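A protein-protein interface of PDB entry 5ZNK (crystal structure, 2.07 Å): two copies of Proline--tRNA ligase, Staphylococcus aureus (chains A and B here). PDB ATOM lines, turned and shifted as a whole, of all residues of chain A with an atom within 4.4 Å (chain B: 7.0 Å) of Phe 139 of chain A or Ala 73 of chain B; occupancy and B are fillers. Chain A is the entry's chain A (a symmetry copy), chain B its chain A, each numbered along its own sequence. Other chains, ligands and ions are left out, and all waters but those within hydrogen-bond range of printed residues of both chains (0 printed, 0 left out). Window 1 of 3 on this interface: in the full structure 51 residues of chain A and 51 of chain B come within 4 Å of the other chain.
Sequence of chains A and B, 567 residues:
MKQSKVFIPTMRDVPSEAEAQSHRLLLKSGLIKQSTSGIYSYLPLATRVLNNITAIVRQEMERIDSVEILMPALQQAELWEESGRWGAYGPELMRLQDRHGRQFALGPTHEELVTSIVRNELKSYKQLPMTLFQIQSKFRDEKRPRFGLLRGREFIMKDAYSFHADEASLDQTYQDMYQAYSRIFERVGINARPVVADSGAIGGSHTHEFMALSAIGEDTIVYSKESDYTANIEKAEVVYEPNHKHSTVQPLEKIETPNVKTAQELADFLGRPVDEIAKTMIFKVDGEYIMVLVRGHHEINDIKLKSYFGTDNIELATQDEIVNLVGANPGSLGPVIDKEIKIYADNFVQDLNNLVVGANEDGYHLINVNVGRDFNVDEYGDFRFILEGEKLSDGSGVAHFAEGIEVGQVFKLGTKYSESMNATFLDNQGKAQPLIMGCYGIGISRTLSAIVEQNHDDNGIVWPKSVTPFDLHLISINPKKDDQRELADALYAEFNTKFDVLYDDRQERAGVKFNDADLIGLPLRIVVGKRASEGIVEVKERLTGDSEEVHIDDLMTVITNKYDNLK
N of Ala 73 of chain B is in hydrogen-bond range of OE2 of Glu 154 of chain A (2.9 Å). The backbone NH (N) of Leu 74 of chain B is in hydrogen-bond range of the side-chain carboxylate (OE1) of Glu 154 of chain A, 3.0 Å away.
O of Ala 73 of chain B lies within hydrogen-bond range of N of Gly 107 of chain B (2.8 Å). O of Leu 96 of chain B is in hydrogen-bond range of N of Phe 104 of chain B, 2.7 Å away. N of Gly 107 of chain A is in hydrogen-bond range of O of Ala 73 of chain A (2.8 Å). The backbone carbonyl oxygen of Met 94 of chain A lies within hydrogen-bond range of the backbone NH of Leu 106 of chain A (3.0 Å). The backbone carbonyl oxygen (O) of Gly 107 of chain A lies within hydrogen-bond range of the backbone NH (N) of Phe 139 of chain A (2.9 Å). N of Arg 140 of chain A sits at hydrogen-bond distance from O of Arg 153 of chain A (2.9 Å).
Among the printed residues, merely in contact across the chains: Ala 73 of chain A with Phe 139 of chain B (3.9 Å), Met 94 of chain A with Leu 74 of chain B (3.8 Å), Met 94 of chain A with Leu 96 of chain B (3.9 Å), Leu 106 of chain A with Leu 96 of chain B (3.8 Å), Leu 106 of chain A with Leu 106 of chain B (3.9 Å), Phe 139 of chain A with Ala 73 of chain B (3.9 Å), Phe 139 of chain A with Leu 74 of chain B (3.7 Å), Arg 153 of chain A with Phe 104 of chain B (3.8 Å) and Glu 154 of chain A with Pro 72 of chain B (3.5 Å).
Phe 139 of chain A touches two residues of chain B. Of chain A, only Phe 139 and Glu 154 come within 4 Å of Ala 73 of chain B. Of the printed residues of chain B, Arg 153 of chain A touches Phe 104. Of the printed residues of chain B, Leu 106 of chain A touches Leu 96 (3.8 Å) and Leu 106 (3.9 Å). Printed residues of chain A within 4 Å of Pro 72 of chain B: Glu 154. Pro 108 of chain A touches none of the printed residues of chain B. The nearest residue of chain B that does not touch Phe 139 of chain A is Leu 106 of chain B (5.0 Å). The nearest printed residue of chain B that does not touch Leu 106 of chain A is Leu 74 of chain B (4.3 Å).
Printed residues of chain A that touch a printed residue of chain B: Ala 73, Met 94, Leu 106, Phe 139, Arg 153 and Glu 154. Hydrophobic or aromatic side chains of chain A that line the printed part of chain B: Ala 73, Met 94, Leu 106 and Phe 139. Along chain B the printed residues that touch a printed residue of chain A span positions 72 to 139. Among the printed residues, 11 pairs touch across the chains. Among the printed residues, no Asp or Glu carboxylate lies within 4 Å of a Lys or Arg side-chain nitrogen of the other chain.
Ala 73 of chain A touches Phe 139 of chain B, and with the chains exchanged Phe 139 of chain A touches Ala 73 of chain B. Leu 106 of chain B touches its own counterpart, Leu 106 of chain A. Positions printed for both chains: 73, 106, 107, 108, 137, 138 and 139. Of the 11 pairs that touch across the chains among the printed residues, 3 have their exchanged pair printed and touching as well.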
ATOM      1  N   ALA A  73      37.194  27.929  -4.126  1.00  0.00           N
ATOM      2  CA  ALA A  73      36.442  27.274  -3.042  1.00  0.00           C
ATOM      3  C   ALA A  73      36.516  25.741  -3.097  1.00  0.00           C
ATOM      4  O   ALA A  73      36.574  25.080  -2.057  1.00  0.00           O
ATOM      5  CB  ALA A  73      34.986  27.711  -3.091  1.00  0.00           C
ATOM      6  N   MET A  94      32.827  21.163   5.124  1.00  0.00           N
ATOM      7  CA  MET A  94      31.798  20.789   4.163  1.00  0.00           C
ATOM      8  C   MET A  94      32.478  20.028   3.042  1.00  0.00           C
ATOM      9  O   MET A  94      33.481  20.490   2.526  1.00  0.00           O
ATOM     10  CB  MET A  94      31.070  22.015   3.626  1.00  0.00           C
ATOM     11  CG  MET A  94      30.381  22.823   4.716  1.00  0.00           C
ATOM     12  SD  MET A  94      29.167  24.007   4.117  1.00  0.00           S
ATOM     13  CE  MET A  94      27.808  22.885   3.760  1.00  0.00           C
ATOM     14  N   LEU A 106      34.737  22.178   0.381  1.00  0.00           N
ATOM     15  CA  LEU A 106      34.544  23.626   0.206  1.00  0.00           C
ATOM     16  C   LEU A 106      35.450  24.315   1.206  1.00  0.00           C
ATOM     17  O   LEU A 106      35.430  23.974   2.397  1.00  0.00           O
ATOM     18  CB  LEU A 106      33.105  24.047   0.456  1.00  0.00           C
ATOM     19  CG  LEU A 106      32.069  23.556  -0.554  1.00  0.00           C
ATOM     20  CD1 LEU A 106      30.659  23.850  -0.060  1.00  0.00           C
ATOM     21  CD2 LEU A 106      32.315  24.196  -1.911  1.00  0.00           C
ATOM     22  N   GLY A 107      36.240  25.278   0.739  1.00  0.00           N
ATOM     23  CA  GLY A 107      37.302  25.860   1.559  1.00  0.00           C
ATOM     24  C   GLY A 107      36.770  26.551   2.809  1.00  0.00           C
ATOM     25  O   GLY A 107      35.967  27.473   2.688  1.00  0.00           O
ATOM     26  N   PRO A 108      37.192  26.097   4.013  1.00  0.00           N
ATOM     27  CA  PRO A 108      36.972  26.859   5.249  1.00  0.00           C
ATOM     28  C   PRO A 108      38.089  27.857   5.536  1.00  0.00           C
ATOM     29  O   PRO A 108      37.934  28.737   6.382  1.00  0.00           O
ATOM     30  CB  PRO A 108      36.946  25.768   6.325  1.00  0.00           C
ATOM     31  CG  PRO A 108      37.885  24.741   5.805  1.00  0.00           C
ATOM     32  CD  PRO A 108      37.801  24.783   4.301  1.00  0.00           C
ATOM     33  N   SER A 137      34.909  33.965  -0.215  1.00  0.00           N
ATOM     34  CA  SER A 137      33.894  33.380   0.635  1.00  0.00           C
ATOM     35  C   SER A 137      34.307  32.018   1.124  1.00  0.00           C
ATOM     36  O   SER A 137      34.716  31.169   0.332  1.00  0.00           O
ATOM     37  CB  SER A 137      32.556  33.357  -0.075  1.00  0.00           C
ATOM     38  OG  SER A 137      32.057  34.682  -0.059  1.00  0.00           O
ATOM     39  N   LYS A 138      34.259  31.848   2.444  1.00  0.00           N
ATOM     40  CA  LYS A 138      34.589  30.583   3.118  1.00  0.00           C
ATOM     41  C   LYS A 138      33.328  29.876   3.539  1.00  0.00           C
ATOM     42  O   LYS A 138      32.278  30.498   3.720  1.00  0.00           O
ATOM     43  CB  LYS A 138      35.396  30.822   4.378  1.00  0.00           C
ATOM     44  CG  LYS A 138      36.626  31.680   4.184  1.00  0.00           C
ATOM     45  CD  LYS A 138      37.703  30.999   3.347  1.00  0.00           C
ATOM     46  CE  LYS A 138      38.875  31.938   3.166  1.00  0.00           C
ATOM     47  NZ  LYS A 138      38.628  32.908   2.073  1.00  0.00           N
ATOM     48  N   PHE A 139      33.486  28.578   3.758  1.00  0.00           N
ATOM     49  CA  PHE A 139      32.419  27.661   4.064  1.00  0.00           C
ATOM     50  C   PHE A 139      32.796  26.877   5.304  1.00  0.00           C
ATOM     51  O   PHE A 139      33.825  26.206   5.318  1.00  0.00           O
ATOM     52  CB  PHE A 139      32.217  26.700   2.888  1.00  0.00           C
ATOM     53  CG  PHE A 139      31.795  27.385   1.627  1.00  0.00           C
ATOM     54  CD1 PHE A 139      32.752  27.856   0.729  1.00  0.00           C
ATOM     55  CD2 PHE A 139      30.456  27.615   1.354  1.00  0.00           C
ATOM     56  CE1 PHE A 139      32.377  28.518  -0.443  1.00  0.00           C
ATOM     57  CE2 PHE A 139      30.067  28.267   0.176  1.00  0.00           C
ATOM     58  CZ  PHE A 139      31.030  28.715  -0.721  1.00  0.00           C
ATOM     59  N   ARG A 140      31.983  26.993   6.352  1.00  0.00           N
ATOM     60  CA  ARG A 140      32.142  26.198   7.570  1.00  0.00           C
ATOM     61  C   ARG A 140      30.780  25.788   8.093  1.00  0.00           C
ATOM     62  O   ARG A 140      29.926  26.638   8.332  1.00  0.00           O
ATOM     63  CB  ARG A 140      32.869  26.998   8.635  1.00  0.00           C
ATOM     64  CG  ARG A 140      34.288  27.359   8.253  1.00  0.00           C
ATOM     65  CD  ARG A 140      34.961  28.124   9.357  1.00  0.00           C
ATOM     66  NE  ARG A 140      36.278  28.560   8.943  1.00  0.00           N
ATOM     67  CZ  ARG A 140      37.118  29.249   9.703  1.00  0.00           C
ATOM     68  NH1 ARG A 140      36.793  29.593  10.939  1.00  0.00           N
ATOM     69  NH2 ARG A 140      38.297  29.581   9.227  1.00  0.00           N
ATOM     70  N   ARG A 153      27.543  30.302   7.993  1.00  0.00           N
ATOM     71  CA  ARG A 153      28.121  29.106   7.391  1.00  0.00           C
ATOM     72  C   ARG A 153      28.803  29.392   6.063  1.00  0.00           C
ATOM     73  O   ARG A 153      29.684  28.654   5.666  1.00  0.00           O
ATOM     74  CB  ARG A 153      27.050  28.044   7.190  1.00  0.00           C
ATOM     75  CG  ARG A 153      26.417  27.598   8.499  1.00  0.00           C
ATOM     76  CD  ARG A 153      25.696  26.275   8.326  1.00  0.00           C
ATOM     77  NE  ARG A 153      24.379  26.439   7.715  1.00  0.00           N
ATOM     78  CZ  ARG A 153      23.624  25.451   7.238  1.00  0.00           C
ATOM     79  NH1 ARG A 153      24.036  24.176   7.264  1.00  0.00           N
ATOM     80  NH2 ARG A 153      22.431  25.741   6.737  1.00  0.00           N
ATOM     81  N   GLU A 154      28.359  30.444   5.380  1.00  0.00           N
ATOM     82  CA  GLU A 154      29.071  31.016   4.247  1.00  0.00           C
ATOM     83  C   GLU A 154      29.356  32.458   4.633  1.00  0.00           C
ATOM     84  O   GLU A 154      28.436  33.185   4.973  1.00  0.00           O
ATOM     85  CB  GLU A 154      28.214  30.944   2.978  1.00  0.00           C
ATOM     86  CG  GLU A 154      28.957  31.387   1.712  1.00  0.00           C
ATOM     87  CD  GLU A 154      28.155  31.168   0.426  1.00  0.00           C
ATOM     88  OE1 GLU A 154      27.272  30.271   0.391  1.00  0.00           O
ATOM     89  OE2 GLU A 154      28.409  31.900  -0.557  1.00  0.00           O
ATOM     90  N   MET B  71      24.885  37.205  -3.625  1.00  0.00           N
ATOM     91  CA  MET B  71      24.054  36.082  -3.218  1.00  0.00           C
ATOM     92  C   MET B  71      24.948  34.894  -2.921  1.00  0.00           C
ATOM     93  O   MET B  71      26.067  34.835  -3.417  1.00  0.00           O
ATOM     94  CB  MET B  71      23.041  35.727  -4.310  1.00  0.00           C
ATOM     95  CG  MET B  71      22.005  36.817  -4.559  1.00  0.00           C
ATOM     96  SD  MET B  71      20.849  36.342  -5.857  1.00  0.00           S
ATOM     97  CE  MET B  71      21.761  36.802  -7.321  1.00  0.00           C
ATOM     98  N   PRO B  72      24.455  33.955  -2.091  1.00  0.00           N
ATOM     99  CA  PRO B  72      25.264  32.828  -1.659  1.00  0.00           C
ATOM    100  C   PRO B  72      25.464  31.752  -2.722  1.00  0.00           C
ATOM    101  O   PRO B  72      24.586  31.539  -3.551  1.00  0.00           O
ATOM    102  CB  PRO B  72      24.445  32.249  -0.488  1.00  0.00           C
ATOM    103  CG  PRO B  72      23.042  32.655  -0.768  1.00  0.00           C
ATOM    104  CD  PRO B  72      23.193  34.036  -1.324  1.00  0.00           C
ATOM    105  N   ALA B  73      26.604  31.073  -2.666  1.00  0.00           N
ATOM    106  CA  ALA B  73      26.839  29.842  -3.440  1.00  0.00           C
ATOM    107  C   ALA B  73      26.017  28.647  -2.939  1.00  0.00           C
ATOM    108  O   ALA B  73      25.553  27.827  -3.736  1.00  0.00           O
ATOM    109  CB  ALA B  73      28.319  29.488  -3.406  1.00  0.00           C
ATOM    110  N   LEU B  74      25.868  28.528  -1.625  1.00  0.00           N
ATOM    111  CA  LEU B  74      25.109  27.415  -1.041  1.00  0.00           C
ATOM    112  C   LEU B  74      23.629  27.703  -1.143  1.00  0.00           C
ATOM    113  O   LEU B  74      23.156  28.662  -0.545  1.00  0.00           O
ATOM    114  CB  LEU B  74      25.485  27.184   0.428  1.00  0.00           C
ATOM    115  CG  LEU B  74      26.733  26.350   0.671  1.00  0.00           C
ATOM    116  CD1 LEU B  74      27.088  26.441   2.153  1.00  0.00           C
ATOM    117  CD2 LEU B  74      26.504  24.893   0.258  1.00  0.00           C
ATOM    118  N   GLN B  75      22.923  26.874  -1.910  1.00  0.00           N
ATOM    119  CA  GLN B  75      21.512  27.074  -2.201  1.00  0.00           C
ATOM    120  C   GLN B  75      20.764  25.811  -1.830  1.00  0.00           C
ATOM    121  O   GLN B  75      21.055  24.729  -2.353  1.00  0.00           O
ATOM    122  CB  GLN B  75      21.304  27.375  -3.668  1.00  0.00           C
ATOM    123  CG  GLN B  75      22.112  28.563  -4.151  1.00  0.00           C
ATOM    124  CD  GLN B  75      21.806  28.954  -5.573  1.00  0.00           C
ATOM    125  OE1 GLN B  75      20.886  28.438  -6.198  1.00  0.00           O
ATOM    126  NE2 GLN B  75      22.597  29.875  -6.098  1.00  0.00           N
ATOM    127  N   GLN B  76      19.816  25.953  -0.915  1.00  0.00           N
ATOM    128  CA  GLN B  76      19.055  24.818  -0.421  1.00  0.00           C
ATOM    129  C   GLN B  76      18.258  24.172  -1.551  1.00  0.00           C
ATOM    130  O   GLN B  76      17.672  24.866  -2.385  1.00  0.00           O
ATOM    131  CB  GLN B  76      18.166  25.236   0.755  1.00  0.00           C
ATOM    132  CG  GLN B  76      17.062  26.213   0.417  1.00  0.00           C
ATOM    133  CD  GLN B  76      16.359  26.738   1.653  1.00  0.00           C
ATOM    134  OE1 GLN B  76      16.388  26.112   2.725  1.00  0.00           O
ATOM    135  NE2 GLN B  76      15.709  27.886   1.511  1.00  0.00           N
ATOM    136  N   LEU B  96      25.409  18.663  -2.503  1.00  0.00           N
ATOM    137  CA  LEU B  96      25.999  18.194  -1.256  1.00  0.00           C
ATOM    138  C   LEU B  96      24.969  18.197  -0.128  1.00  0.00           C
ATOM    139  O   LEU B  96      23.855  18.681  -0.294  1.00  0.00           O
ATOM    140  CB  LEU B  96      27.231  19.031  -0.879  1.00  0.00           C
ATOM    141  CG  LEU B  96      27.025  20.473  -0.388  1.00  0.00           C
ATOM    142  CD1 LEU B  96      28.208  20.936   0.428  1.00  0.00           C
ATOM    143  CD2 LEU B  96      26.802  21.423  -1.546  1.00  0.00           C
ATOM    144  N   PHE B 104      21.869  20.571  -0.502  1.00  0.00           N
ATOM    145  CA  PHE B 104      22.181  21.837  -1.162  1.00  0.00           C
ATOM    146  C   PHE B 104      22.712  21.647  -2.578  1.00  0.00           C
ATOM    147  O   PHE B 104      23.271  20.610  -2.919  1.00  0.00           O
ATOM    148  CB  PHE B 104      23.242  22.606  -0.370  1.00  0.00           C
ATOM    149  CG  PHE B 104      22.750  23.157   0.930  1.00  0.00           C
ATOM    150  CD1 PHE B 104      22.720  22.363   2.066  1.00  0.00           C
ATOM    151  CD2 PHE B 104      22.324  24.469   1.023  1.00  0.00           C
ATOM    152  CE1 PHE B 104      22.257  22.866   3.271  1.00  0.00           C
ATOM    153  CE2 PHE B 104      21.876  24.985   2.227  1.00  0.00           C
ATOM    154  CZ  PHE B 104      21.831  24.180   3.350  1.00  0.00           C
ATOM    155  N   ALA B 105      22.547  22.693  -3.377  1.00  0.00           N
ATOM    156  CA  ALA B 105      23.285  22.876  -4.621  1.00  0.00           C
ATOM    157  C   ALA B 105      24.327  23.980  -4.421  1.00  0.00           C
ATOM    158  O   ALA B 105      24.076  24.945  -3.690  1.00  0.00           O
ATOM    159  CB  ALA B 105      22.328  23.275  -5.731  1.00  0.00           C
ATOM    160  N   LEU B 106      25.496  23.823  -5.041  1.00  0.00           N
ATOM    161  CA  LEU B 106      26.397  24.959  -5.290  1.00  0.00           C
ATOM    162  C   LEU B 106      25.876  25.674  -6.520  1.00  0.00           C
ATOM    163  O   LEU B 106      25.627  25.031  -7.550  1.00  0.00           O
ATOM    164  CB  LEU B 106      27.829  24.511  -5.535  1.00  0.00           C
ATOM    165  CG  LEU B 106      28.562  23.896  -4.344  1.00  0.00           C
ATOM    166  CD1 LEU B 106      29.886  23.287  -4.786  1.00  0.00           C
ATOM    167  CD2 LEU B 106      28.779  24.944  -3.264  1.00  0.00           C
ATOM    168  N   GLY B 107      25.712  26.991  -6.427  1.00  0.00           N
ATOM    169  CA  GLY B 107      25.018  27.749  -7.466  1.00  0.00           C
ATOM    170  C   GLY B 107      25.719  27.675  -8.818  1.00  0.00           C
ATOM    171  O   GLY B 107      26.881  28.062  -8.911  1.00  0.00           O
ATOM    172  N   PRO B 108      25.031  27.157  -9.863  1.00  0.00           N
ATOM    173  CA  PRO B 108      25.498  27.300 -11.247  1.00  0.00           C
ATOM    174  C   PRO B 108      25.007  28.584 -11.908  1.00  0.00           C
ATOM    175  O   PRO B 108      25.510  28.971 -12.962  1.00  0.00           O
ATOM    176  CB  PRO B 108      24.890  26.078 -11.944  1.00  0.00           C
ATOM    177  CG  PRO B 108      23.610  25.863 -11.220  1.00  0.00           C
ATOM    178  CD  PRO B 108      23.827  26.303  -9.795  1.00  0.00           C
ATOM    179  N   HIS B 110      21.567  31.767 -10.539  1.00  0.00           N
ATOM    180  CA  HIS B 110      20.819  32.221  -9.352  1.00  0.00           C
ATOM    181  C   HIS B 110      19.366  32.682  -9.593  1.00  0.00           C
ATOM    182  O   HIS B 110      18.870  33.533  -8.861  1.00  0.00           O
ATOM    183  CB  HIS B 110      21.624  33.324  -8.632  1.00  0.00           C
ATOM    184  CG  HIS B 110      22.891  32.841  -8.002  1.00  0.00           C
ATOM    185  ND1 HIS B 110      23.127  32.923  -6.647  1.00  0.00           N
ATOM    186  CD2 HIS B 110      23.990  32.267  -8.539  1.00  0.00           C
ATOM    187  CE1 HIS B 110      24.322  32.422  -6.378  1.00  0.00           C
ATOM    188  NE2 HIS B 110      24.857  31.998  -7.506  1.00  0.00           N
ATOM    189  N   LEU B 113      17.335  31.806  -6.417  1.00  0.00           N
ATOM    190  CA  LEU B 113      17.841  32.554  -5.268  1.00  0.00           C
ATOM    191  C   LEU B 113      17.375  34.007  -5.335  1.00  0.00           C
ATOM    192  O   LEU B 113      16.837  34.521  -4.364  1.00  0.00           O
ATOM    193  CB  LEU B 113      19.373  32.467  -5.174  1.00  0.00           C
ATOM    194  CG  LEU B 113      20.039  32.569  -3.787  1.00  0.00           C
ATOM    195  CD1 LEU B 113      19.600  33.801  -3.031  1.00  0.00           C
ATOM    196  CD2 LEU B 113      19.738  31.344  -2.936  1.00  0.00           C
ATOM    197  N   GLN B 134      25.165  40.571  -9.569  1.00  0.00           N
ATOM    198  CA  GLN B 134      26.307  40.220  -8.751  1.00  0.00           C
ATOM    199  C   GLN B 134      27.463  39.797  -9.647  1.00  0.00           C
ATOM    200  O   GLN B 134      27.278  39.487 -10.834  1.00  0.00           O
ATOM    201  CB  GLN B 134      25.957  39.097  -7.764  1.00  0.00           C
ATOM    202  CG  GLN B 134      25.487  37.816  -8.411  1.00  0.00           C
ATOM    203  CD  GLN B 134      25.390  36.624  -7.472  1.00  0.00           C
ATOM    204  OE1 GLN B 134      25.697  36.693  -6.268  1.00  0.00           O
ATOM    205  NE2 GLN B 134      24.980  35.497  -8.035  1.00  0.00           N
ATOM    206  N   GLN B 136      30.137  36.919  -9.048  1.00  0.00           N
ATOM    207  CA  GLN B 136      30.217  35.848  -8.082  1.00  0.00           C
ATOM    208  C   GLN B 136      30.619  34.562  -8.762  1.00  0.00           C
ATOM    209  O   GLN B 136      30.365  34.361  -9.949  1.00  0.00           O
ATOM    210  CB  GLN B 136      28.864  35.727  -7.379  1.00  0.00           C
ATOM    211  CG  GLN B 136      28.786  34.795  -6.169  1.00  0.00           C
ATOM    212  CD  GLN B 136      28.135  33.453  -6.477  1.00  0.00           C
ATOM    213  OE1 GLN B 136      27.704  33.182  -7.604  1.00  0.00           O
ATOM    214  NE2 GLN B 136      28.064  32.601  -5.474  1.00  0.00           N
ATOM    215  N   SER B 137      31.263  33.689  -7.996  1.00  0.00           N
ATOM    216  CA  SER B 137      31.778  32.454  -8.548  1.00  0.00           C
ATOM    217  C   SER B 137      30.704  31.405  -8.641  1.00  0.00           C
ATOM    218  O   SER B 137      29.993  31.152  -7.668  1.00  0.00           O
ATOM    219  CB  SER B 137      32.981  31.981  -7.756  1.00  0.00           C
ATOM    220  OG  SER B 137      34.070  32.807  -8.125  1.00  0.00           O
ATOM    221  N   LYS B 138      30.554  30.849  -9.843  1.00  0.00           N
ATOM    222  CA  LYS B 138      29.584  29.782 -10.134  1.00  0.00           C
ATOM    223  C   LYS B 138      30.286  28.453 -10.221  1.00  0.00           C
ATOM    224  O   LYS B 138      31.488  28.384 -10.493  1.00  0.00           O
ATOM    225  CB  LYS B 138      28.902  30.003 -11.469  1.00  0.00           C
ATOM    226  CG  LYS B 138      28.283  31.372 -11.640  1.00  0.00           C
ATOM    227  CD  LYS B 138      27.083  31.603 -10.730  1.00  0.00           C
ATOM    228  CE  LYS B 138      26.553  33.005 -10.933  1.00  0.00           C
ATOM    229  NZ  LYS B 138      27.339  33.998 -10.162  1.00  0.00           N
ATOM    230  N   PHE B 139      29.486  27.410 -10.056  1.00  0.00           N
ATOM    231  CA  PHE B 139      29.926  26.040  -9.987  1.00  0.00           C
ATOM    232  C   PHE B 139      29.109  25.220 -10.964  1.00  0.00           C
ATOM    233  O   PHE B 139      27.885  25.181 -10.861  1.00  0.00           O
ATOM    234  CB  PHE B 139      29.718  25.507  -8.566  1.00  0.00           C
ATOM    235  CG  PHE B 139      30.526  26.230  -7.536  1.00  0.00           C
ATOM    236  CD1 PHE B 139      30.007  27.357  -6.900  1.00  0.00           C
ATOM    237  CD2 PHE B 139      31.819  25.832  -7.235  1.00  0.00           C
ATOM    238  CE1 PHE B 139      30.757  28.059  -5.952  1.00  0.00           C
ATOM    239  CE2 PHE B 139      32.576  26.520  -6.277  1.00  0.00           C
ATOM    240  CZ  PHE B 139      32.040  27.631  -5.636  1.00  0.00           C
